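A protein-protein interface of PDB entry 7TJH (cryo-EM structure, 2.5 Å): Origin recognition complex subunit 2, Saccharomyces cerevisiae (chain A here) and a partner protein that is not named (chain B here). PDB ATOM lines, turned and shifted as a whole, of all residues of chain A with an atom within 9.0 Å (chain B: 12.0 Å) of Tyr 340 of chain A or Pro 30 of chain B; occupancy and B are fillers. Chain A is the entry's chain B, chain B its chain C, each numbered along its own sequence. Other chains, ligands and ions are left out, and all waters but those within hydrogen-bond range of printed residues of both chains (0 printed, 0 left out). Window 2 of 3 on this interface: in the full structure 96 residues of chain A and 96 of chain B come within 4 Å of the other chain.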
ATOM      1  N   TRP A 305     -23.196 -24.407   8.226  1.00  0.00           N
ATOM      2  CA  TRP A 305     -23.642 -25.132   7.038  1.00  0.00           C
ATOM      3  C   TRP A 305     -22.813 -26.397   6.818  1.00  0.00           C
ATOM      4  O   TRP A 305     -23.361 -27.456   6.482  1.00  0.00           O
ATOM      5  CB  TRP A 305     -23.588 -24.185   5.831  1.00  0.00           C
ATOM      6  CG  TRP A 305     -23.888 -24.765   4.469  1.00  0.00           C
ATOM      7  CD1 TRP A 305     -24.659 -25.852   4.173  1.00  0.00           C
ATOM      8  CD2 TRP A 305     -23.428 -24.252   3.214  1.00  0.00           C
ATOM      9  NE1 TRP A 305     -24.687 -26.060   2.819  1.00  0.00           N
ATOM     10  CE2 TRP A 305     -23.942 -25.088   2.205  1.00  0.00           C
ATOM     11  CE3 TRP A 305     -22.632 -23.164   2.846  1.00  0.00           C
ATOM     12  CZ2 TRP A 305     -23.681 -24.873   0.854  1.00  0.00           C
ATOM     13  CZ3 TRP A 305     -22.367 -22.959   1.505  1.00  0.00           C
ATOM     14  CH2 TRP A 305     -22.893 -23.806   0.526  1.00  0.00           C
ATOM     15  N   ILE A 331     -32.978 -18.742   7.057  1.00  0.00           N
ATOM     16  CA  ILE A 331     -33.737 -18.211   5.934  1.00  0.00           C
ATOM     17  C   ILE A 331     -32.844 -17.420   4.985  1.00  0.00           C
ATOM     18  O   ILE A 331     -32.817 -17.686   3.783  1.00  0.00           O
ATOM     19  CB  ILE A 331     -34.926 -17.355   6.431  1.00  0.00           C
ATOM     20  CG1 ILE A 331     -36.050 -18.259   6.933  1.00  0.00           C
ATOM     21  CG2 ILE A 331     -35.477 -16.462   5.327  1.00  0.00           C
ATOM     22  CD1 ILE A 331     -36.816 -17.681   8.091  1.00  0.00           C
ATOM     23  N   ASP A 332     -32.091 -16.446   5.513  1.00  0.00           N
ATOM     24  CA  ASP A 332     -31.311 -15.582   4.637  1.00  0.00           C
ATOM     25  C   ASP A 332     -30.057 -16.275   4.123  1.00  0.00           C
ATOM     26  O   ASP A 332     -29.546 -15.916   3.058  1.00  0.00           O
ATOM     27  CB  ASP A 332     -30.938 -14.291   5.364  1.00  0.00           C
ATOM     28  CG  ASP A 332     -32.149 -13.546   5.878  1.00  0.00           C
ATOM     29  OD1 ASP A 332     -33.266 -13.813   5.388  1.00  0.00           O
ATOM     30  OD2 ASP A 332     -31.983 -12.681   6.760  1.00  0.00           O
ATOM     31  N   TYR A 333     -29.547 -17.264   4.855  1.00  0.00           N
ATOM     32  CA  TYR A 333     -28.297 -17.912   4.488  1.00  0.00           C
ATOM     33  C   TYR A 333     -28.488 -19.372   4.099  1.00  0.00           C
ATOM     34  O   TYR A 333     -28.096 -19.766   3.001  1.00  0.00           O
ATOM     35  CB  TYR A 333     -27.283 -17.788   5.639  1.00  0.00           C
ATOM     36  CG  TYR A 333     -25.899 -18.298   5.293  1.00  0.00           C
ATOM     37  CD1 TYR A 333     -24.987 -17.486   4.631  1.00  0.00           C
ATOM     38  CD2 TYR A 333     -25.502 -19.588   5.632  1.00  0.00           C
ATOM     39  CE1 TYR A 333     -23.724 -17.944   4.311  1.00  0.00           C
ATOM     40  CE2 TYR A 333     -24.244 -20.057   5.308  1.00  0.00           C
ATOM     41  CZ  TYR A 333     -23.360 -19.230   4.652  1.00  0.00           C
ATOM     42  OH  TYR A 333     -22.107 -19.692   4.333  1.00  0.00           O
ATOM     43  N   LEU A 334     -29.078 -20.191   4.974  1.00  0.00           N
ATOM     44  CA  LEU A 334     -28.935 -21.639   4.846  1.00  0.00           C
ATOM     45  C   LEU A 334     -29.778 -22.215   3.714  1.00  0.00           C
ATOM     46  O   LEU A 334     -29.290 -23.041   2.934  1.00  0.00           O
ATOM     47  CB  LEU A 334     -29.290 -22.316   6.168  1.00  0.00           C
ATOM     48  CG  LEU A 334     -29.124 -23.833   6.156  1.00  0.00           C
ATOM     49  CD1 LEU A 334     -27.653 -24.200   6.224  1.00  0.00           C
ATOM     50  CD2 LEU A 334     -29.902 -24.458   7.291  1.00  0.00           C
ATOM     51  N   SER A 335     -31.045 -21.809   3.619  1.00  0.00           N
ATOM     52  CA  SER A 335     -31.898 -22.319   2.548  1.00  0.00           C
ATOM     53  C   SER A 335     -31.446 -21.934   1.132  1.00  0.00           C
ATOM     54  O   SER A 335     -31.441 -22.837   0.275  1.00  0.00           O
ATOM     55  CB  SER A 335     -33.366 -21.942   2.819  1.00  0.00           C
ATOM     56  OG  SER A 335     -33.799 -20.762   2.177  1.00  0.00           O
ATOM     57  N   PRO A 336     -31.028 -20.689   0.806  1.00  0.00           N
ATOM     58  CA  PRO A 336     -30.515 -20.470  -0.558  1.00  0.00           C
ATOM     59  C   PRO A 336     -29.189 -21.160  -0.834  1.00  0.00           C
ATOM     60  O   PRO A 336     -28.986 -21.620  -1.964  1.00  0.00           O
ATOM     61  CB  PRO A 336     -30.377 -18.942  -0.653  1.00  0.00           C
ATOM     62  CG  PRO A 336     -31.163 -18.407   0.452  1.00  0.00           C
ATOM     63  CD  PRO A 336     -31.013 -19.402   1.533  1.00  0.00           C
ATOM     64  N   LYS A 337     -28.298 -21.268   0.160  1.00  0.00           N
ATOM     65  CA  LYS A 337     -27.028 -21.962  -0.050  1.00  0.00           C
ATOM     66  C   LYS A 337     -27.238 -23.449  -0.296  1.00  0.00           C
ATOM     67  O   LYS A 337     -26.589 -24.032  -1.174  1.00  0.00           O
ATOM     68  CB  LYS A 337     -26.096 -21.757   1.144  1.00  0.00           C
ATOM     69  CG  LYS A 337     -25.462 -20.383   1.238  1.00  0.00           C
ATOM     70  CD  LYS A 337     -24.356 -20.188   0.229  1.00  0.00           C
ATOM     71  CE  LYS A 337     -23.397 -19.115   0.702  1.00  0.00           C
ATOM     72  NZ  LYS A 337     -24.061 -17.788   0.801  1.00  0.00           N
ATOM     73  N   ILE A 338     -28.146 -24.076   0.459  1.00  0.00           N
ATOM     74  CA  ILE A 338     -28.434 -25.490   0.247  1.00  0.00           C
ATOM     75  C   ILE A 338     -29.147 -25.695  -1.086  1.00  0.00           C
ATOM     76  O   ILE A 338     -28.826 -26.629  -1.830  1.00  0.00           O
ATOM     77  CB  ILE A 338     -29.232 -26.064   1.437  1.00  0.00           C
ATOM     78  CG1 ILE A 338     -28.327 -26.181   2.665  1.00  0.00           C
ATOM     79  CG2 ILE A 338     -29.814 -27.446   1.117  1.00  0.00           C
ATOM     80  CD1 ILE A 338     -28.994 -26.813   3.864  1.00  0.00           C
ATOM     81  N   ALA A 339     -30.081 -24.800  -1.437  1.00  0.00           N
ATOM     82  CA  ALA A 339     -30.798 -24.922  -2.705  1.00  0.00           C
ATOM     83  C   ALA A 339     -29.869 -24.758  -3.906  1.00  0.00           C
ATOM     84  O   ALA A 339     -30.000 -25.483  -4.898  1.00  0.00           O
ATOM     85  CB  ALA A 339     -31.933 -23.900  -2.760  1.00  0.00           C
ATOM     86  N   TYR A 340     -28.912 -23.829  -3.831  1.00  0.00           N
ATOM     87  CA  TYR A 340     -27.954 -23.676  -4.920  1.00  0.00           C
ATOM     88  C   TYR A 340     -26.893 -24.769  -4.918  1.00  0.00           C
ATOM     89  O   TYR A 340     -26.296 -25.047  -5.964  1.00  0.00           O
ATOM     90  CB  TYR A 340     -27.288 -22.303  -4.852  1.00  0.00           C
ATOM     91  CG  TYR A 340     -28.178 -21.164  -5.277  1.00  0.00           C
ATOM     92  CD1 TYR A 340     -29.034 -21.298  -6.363  1.00  0.00           C
ATOM     93  CD2 TYR A 340     -28.162 -19.955  -4.598  1.00  0.00           C
ATOM     94  CE1 TYR A 340     -29.849 -20.259  -6.759  1.00  0.00           C
ATOM     95  CE2 TYR A 340     -28.974 -18.909  -4.986  1.00  0.00           C
ATOM     96  CZ  TYR A 340     -29.814 -19.068  -6.066  1.00  0.00           C
ATOM     97  OH  TYR A 340     -30.626 -18.029  -6.455  1.00  0.00           O
ATOM     98  N   SER A 341     -26.634 -25.395  -3.769  1.00  0.00           N
ATOM     99  CA  SER A 341     -25.538 -26.354  -3.695  1.00  0.00           C
ATOM    100  C   SER A 341     -25.889 -27.720  -4.270  1.00  0.00           C
ATOM    101  O   SER A 341     -24.979 -28.513  -4.529  1.00  0.00           O
ATOM    102  CB  SER A 341     -25.079 -26.516  -2.244  1.00  0.00           C
ATOM    103  OG  SER A 341     -26.084 -27.122  -1.452  1.00  0.00           O
ATOM    104  N   GLN A 342     -27.170 -28.015  -4.482  1.00  0.00           N
ATOM    105  CA  GLN A 342     -27.608 -29.322  -4.953  1.00  0.00           C
ATOM    106  C   GLN A 342     -28.114 -29.285  -6.390  1.00  0.00           C
ATOM    107  O   GLN A 342     -28.930 -30.127  -6.779  1.00  0.00           O
ATOM    108  CB  GLN A 342     -28.681 -29.876  -4.014  1.00  0.00           C
ATOM    109  CG  GLN A 342     -28.317 -29.704  -2.556  1.00  0.00           C
ATOM    110  CD  GLN A 342     -29.330 -30.294  -1.604  1.00  0.00           C
ATOM    111  OE1 GLN A 342     -29.029 -31.221  -0.853  1.00  0.00           O
ATOM    112  NE2 GLN A 342     -30.551 -29.788  -1.661  1.00  0.00           N
ATOM    113  N   LEU A 343     -27.651 -28.328  -7.187  1.00  0.00           N
ATOM    114  CA  LEU A 343     -28.047 -28.249  -8.587  1.00  0.00           C
ATOM    115  C   LEU A 343     -26.872 -28.579  -9.502  1.00  0.00           C
ATOM    116  O   LEU A 343     -26.245 -29.631  -9.368  1.00  0.00           O
ATOM    117  CB  LEU A 343     -28.601 -26.863  -8.914  1.00  0.00           C
ATOM    118  CG  LEU A 343     -29.896 -26.461  -8.202  1.00  0.00           C
ATOM    119  CD1 LEU A 343     -30.243 -25.015  -8.510  1.00  0.00           C
ATOM    120  CD2 LEU A 343     -31.038 -27.382  -8.594  1.00  0.00           C
ATOM    121  N   ASN A 356     -36.918 -23.572  -6.647  1.00  0.00           N
ATOM    122  CA  ASN A 356     -37.320 -22.977  -5.378  1.00  0.00           C
ATOM    123  C   ASN A 356     -36.292 -23.262  -4.292  1.00  0.00           C
ATOM    124  O   ASN A 356     -35.453 -24.155  -4.433  1.00  0.00           O
ATOM    125  CB  ASN A 356     -38.689 -23.502  -4.946  1.00  0.00           C
ATOM    126  CG  ASN A 356     -38.647 -24.961  -4.534  1.00  0.00           C
ATOM    127  OD1 ASN A 356     -38.518 -25.852  -5.374  1.00  0.00           O
ATOM    128  ND2 ASN A 356     -38.749 -25.212  -3.235  1.00  0.00           N
ATOM    129  N   SER A 357     -36.361 -22.499  -3.208  1.00  0.00           N
ATOM    130  CA  SER A 357     -35.483 -22.735  -2.077  1.00  0.00           C
ATOM    131  C   SER A 357     -36.039 -23.854  -1.201  1.00  0.00           C
ATOM    132  O   SER A 357     -37.181 -24.294  -1.352  1.00  0.00           O
ATOM    133  CB  SER A 357     -35.291 -21.453  -1.265  1.00  0.00           C
ATOM    134  OG  SER A 357     -36.528 -20.944  -0.804  1.00  0.00           O
ATOM    135  N   ILE A 358     -35.197 -24.330  -0.294  1.00  0.00           N
ATOM    136  CA  ILE A 358     -35.587 -25.393   0.638  1.00  0.00           C
ATOM    137  C   ILE A 358     -36.611 -24.839   1.623  1.00  0.00           C
ATOM    138  O   ILE A 358     -36.387 -23.758   2.198  1.00  0.00           O
ATOM    139  CB  ILE A 358     -34.354 -25.934   1.363  1.00  0.00           C
ATOM    140  CG1 ILE A 358     -33.246 -26.242   0.355  1.00  0.00           C
ATOM    141  CG2 ILE A 358     -34.694 -27.173   2.183  1.00  0.00           C
ATOM    142  CD1 ILE A 358     -33.581 -27.355  -0.619  1.00  0.00           C
ATOM    143  N   TYR B  26     -41.512 -20.542   2.792  1.00  0.00           N
ATOM    144  CA  TYR B  26     -40.913 -20.800   1.489  1.00  0.00           C
ATOM    145  C   TYR B  26     -40.218 -19.520   1.042  1.00  0.00           C
ATOM    146  O   TYR B  26     -40.816 -18.714   0.318  1.00  0.00           O
ATOM    147  CB  TYR B  26     -41.967 -21.241   0.468  1.00  0.00           C
ATOM    148  CG  TYR B  26     -42.906 -22.326   0.957  1.00  0.00           C
ATOM    149  CD1 TYR B  26     -42.592 -23.668   0.788  1.00  0.00           C
ATOM    150  CD2 TYR B  26     -44.114 -22.007   1.574  1.00  0.00           C
ATOM    151  CE1 TYR B  26     -43.444 -24.664   1.231  1.00  0.00           C
ATOM    152  CE2 TYR B  26     -44.971 -22.995   2.023  1.00  0.00           C
ATOM    153  CZ  TYR B  26     -44.631 -24.321   1.845  1.00  0.00           C
ATOM    154  OH  TYR B  26     -45.485 -25.306   2.288  1.00  0.00           O
ATOM    155  N   PRO B  27     -38.973 -19.291   1.457  1.00  0.00           N
ATOM    156  CA  PRO B  27     -38.343 -17.985   1.223  1.00  0.00           C
ATOM    157  C   PRO B  27     -37.902 -17.804  -0.220  1.00  0.00           C
ATOM    158  O   PRO B  27     -37.464 -18.746  -0.884  1.00  0.00           O
ATOM    159  CB  PRO B  27     -37.136 -18.002   2.170  1.00  0.00           C
ATOM    160  CG  PRO B  27     -36.811 -19.433   2.349  1.00  0.00           C
ATOM    161  CD  PRO B  27     -38.057 -20.240   2.114  1.00  0.00           C
ATOM    162  N   SER B  28     -38.020 -16.569  -0.697  1.00  0.00           N
ATOM    163  CA  SER B  28     -37.637 -16.242  -2.061  1.00  0.00           C
ATOM    164  C   SER B  28     -36.121 -16.178  -2.182  1.00  0.00           C
ATOM    165  O   SER B  28     -35.451 -15.516  -1.385  1.00  0.00           O
ATOM    166  CB  SER B  28     -38.257 -14.912  -2.487  1.00  0.00           C
ATOM    167  OG  SER B  28     -37.781 -14.516  -3.761  1.00  0.00           O
ATOM    168  N   LEU B  29     -35.588 -16.866  -3.182  1.00  0.00           N
ATOM    169  CA  LEU B  29     -34.183 -16.921  -3.544  1.00  0.00           C
ATOM    170  C   LEU B  29     -33.930 -16.109  -4.811  1.00  0.00           C
ATOM    171  O   LEU B  29     -34.795 -16.028  -5.689  1.00  0.00           O
ATOM    172  CB  LEU B  29     -33.730 -18.375  -3.748  1.00  0.00           C
ATOM    173  CG  LEU B  29     -34.041 -19.171  -5.021  1.00  0.00           C
ATOM    174  CD1 LEU B  29     -33.104 -20.357  -5.126  1.00  0.00           C
ATOM    175  CD2 LEU B  29     -35.490 -19.642  -5.059  1.00  0.00           C
ATOM    176  N   PRO B  30     -32.754 -15.468  -4.940  1.00  0.00           N
ATOM    177  CA  PRO B  30     -32.503 -14.622  -6.112  1.00  0.00           C
ATOM    178  C   PRO B  30     -32.086 -15.400  -7.359  1.00  0.00           C
ATOM    179  O   PRO B  30     -32.313 -16.606  -7.439  1.00  0.00           O
ATOM    180  CB  PRO B  30     -31.368 -13.714  -5.640  1.00  0.00           C
ATOM    181  CG  PRO B  30     -30.628 -14.543  -4.659  1.00  0.00           C
ATOM    182  CD  PRO B  30     -31.665 -15.372  -3.952  1.00  0.00           C
ATOM    183  N   HIS B  38     -19.826 -22.260  -3.908  1.00  0.00           N
ATOM    184  CA  HIS B  38     -21.027 -23.039  -3.639  1.00  0.00           C
ATOM    185  C   HIS B  38     -20.753 -24.131  -2.606  1.00  0.00           C
ATOM    186  O   HIS B  38     -21.522 -25.082  -2.480  1.00  0.00           O
ATOM    187  CB  HIS B  38     -21.557 -23.665  -4.928  1.00  0.00           C
ATOM    188  CG  HIS B  38     -22.707 -22.922  -5.531  1.00  0.00           C
ATOM    189  ND1 HIS B  38     -23.411 -23.394  -6.619  1.00  0.00           N
ATOM    190  CD2 HIS B  38     -23.263 -21.730  -5.212  1.00  0.00           C
ATOM    191  CE1 HIS B  38     -24.358 -22.530  -6.936  1.00  0.00           C
ATOM    192  NE2 HIS B  38     -24.287 -21.509  -6.101  1.00  0.00           N
ATOM    193  N   ILE B  39     -19.647 -23.997  -1.879  1.00  0.00           N
ATOM    194  CA  ILE B  39     -19.265 -24.965  -0.853  1.00  0.00           C
ATOM    195  C   ILE B  39     -19.083 -24.222   0.469  1.00  0.00           C
ATOM    196  O   ILE B  39     -18.766 -23.024   0.461  1.00  0.00           O
ATOM    197  CB  ILE B  39     -17.999 -25.746  -1.260  1.00  0.00           C
ATOM    198  CG1 ILE B  39     -16.810 -24.805  -1.478  1.00  0.00           C
ATOM    199  CG2 ILE B  39     -18.270 -26.629  -2.480  1.00  0.00           C
ATOM    200  CD1 ILE B  39     -15.594 -25.482  -2.080  1.00  0.00           C
ATOM    201  N   PRO B  40     -19.290 -24.869   1.623  1.00  0.00           N
ATOM    202  CA  PRO B  40     -19.148 -24.157   2.905  1.00  0.00           C
ATOM    203  C   PRO B  40     -17.717 -23.877   3.332  1.00  0.00           C
ATOM    204  O   PRO B  40     -17.522 -23.315   4.414  1.00  0.00           O
ATOM    205  CB  PRO B  40     -19.830 -25.093   3.917  1.00  0.00           C
ATOM    206  CG  PRO B  40     -20.053 -26.363   3.242  1.00  0.00           C
ATOM    207  CD  PRO B  40     -19.948 -26.180   1.774  1.00  0.00           C
ATOM    208  N   GLU B  55     -11.417 -25.814  -3.297  1.00  0.00           N
ATOM    209  CA  GLU B  55     -12.140 -26.910  -3.941  1.00  0.00           C
ATOM    210  C   GLU B  55     -11.457 -28.258  -3.716  1.00  0.00           C
ATOM    211  O   GLU B  55     -12.125 -29.258  -3.412  1.00  0.00           O
ATOM    212  CB  GLU B  55     -12.290 -26.629  -5.436  1.00  0.00           C
ATOM    213  CG  GLU B  55     -12.998 -27.721  -6.232  1.00  0.00           C
ATOM    214  CD  GLU B  55     -14.512 -27.577  -6.240  1.00  0.00           C
ATOM    215  OE1 GLU B  55     -15.132 -27.590  -5.155  1.00  0.00           O
ATOM    216  OE2 GLU B  55     -15.086 -27.452  -7.342  1.00  0.00           O
ATOM    217  N   TRP B  58     -11.981 -29.423  -0.192  1.00  0.00           N
ATOM    218  CA  TRP B  58     -13.305 -30.030  -0.089  1.00  0.00           C
ATOM    219  C   TRP B  58     -13.304 -31.458  -0.630  1.00  0.00           C
ATOM    220  O   TRP B  58     -13.851 -32.379  -0.001  1.00  0.00           O
ATOM    221  CB  TRP B  58     -14.295 -29.144  -0.844  1.00  0.00           C
ATOM    222  CG  TRP B  58     -15.702 -29.618  -0.956  1.00  0.00           C
ATOM    223  CD1 TRP B  58     -16.300 -30.159  -2.056  1.00  0.00           C
ATOM    224  CD2 TRP B  58     -16.716 -29.526   0.048  1.00  0.00           C
ATOM    225  NE1 TRP B  58     -17.617 -30.438  -1.789  1.00  0.00           N
ATOM    226  CE2 TRP B  58     -17.897 -30.057  -0.504  1.00  0.00           C
ATOM    227  CE3 TRP B  58     -16.735 -29.059   1.365  1.00  0.00           C
ATOM    228  CZ2 TRP B  58     -19.088 -30.128   0.214  1.00  0.00           C
ATOM    229  CZ3 TRP B  58     -17.913 -29.139   2.077  1.00  0.00           C
ATOM    230  CH2 TRP B  58     -19.071 -29.674   1.504  1.00  0.00           C
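Of the 17 printed residues of chain A, 8 touch a printed residue of chain B.
Of the 10 printed residues of chain B, 6 touch a printed residue of chain A.
Hydrophobic or aromatic side chains of chain B that line the printed part of chain A: Pro 27, Leu 29, Pro 30, His 38 and Pro 40.
Among the printed residues, no Asp or Glu carboxylate lies within 4 Å of a Lys or Arg side-chain nitrogen of the other chain.
Among the printed residues, pairs that only touch across the chains: Trp 305 of chain A with His 38 of chain B (3.5 Å), Trp 305 of chain A with Ile 39 of chain B (3.7 Å), Trp 305 of chain A with Pro 40 of chain B (3.6 Å), Ile 331 of chain A with Pro 27 of chain B (3.9 Å), Ser 335 of chain A with Pro 27 of chain B (3.3 Å), Tyr 340 of chain A with Leu 29 of chain B (3.6 Å), Ser 341 of chain A with His 38 of chain B (3.8 Å), Asn 356 of chain A with Leu 29 of chain B (3.8 Å), Ser 357 of chain A with Leu 29 of chain B (3.5 Å) and Ile 358 of chain A with Pro 27 of chain B (3.9 Å).
OG of Ser 341 of chain A lies close to O of Lys 337 of chain A (3.1 Å).
The backbone carbonyl oxygen (O) of Ile 338 of chain A is in hydrogen-bond range of the side-chain hydroxyl (OG) of Ser 341 of chain A.
Of the printed residues of chain B, Trp 305 of chain A touches His 38 (3.5 Å), Ile 39 (3.7 Å) and Pro 40 (3.6 Å).
Of the printed residues of chain B, Ser 335 of chain A touches Pro 27 (3.3 Å).
No residue of chain B comes within 4 Å of Pro 336 of chain A.
Ala 339 of chain A touches none of the printed residues of chain B.
Of chain B, only His 38 comes within 4 Å of Ser 341 of chain A.
No residue of chain B comes within 4 Å of Leu 343 of chain A.
Of the printed residues of chain A, Leu 29 of chain B touches Tyr 340, Asn 356 and Ser 357.
Trp 58 of chain B touches none of the printed residues of chain A.
The nearest residue of chain B that does not touch Tyr 340 of chain A is Ser 28 of chain B (7.2 Å).
OH of Tyr 340 of chain A is in hydrogen-bond range of O of Pro 30 of chain B (2.4 Å).
O of Tyr 340 of chain A lies close to ND1 of His 38 of chain B, 3.4 Å away.
The side-chain hydroxyl (OG) of Ser 357 of chain A lies close to the backbone carbonyl oxygen (O) of Pro 27 of chain B (2.4 Å).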
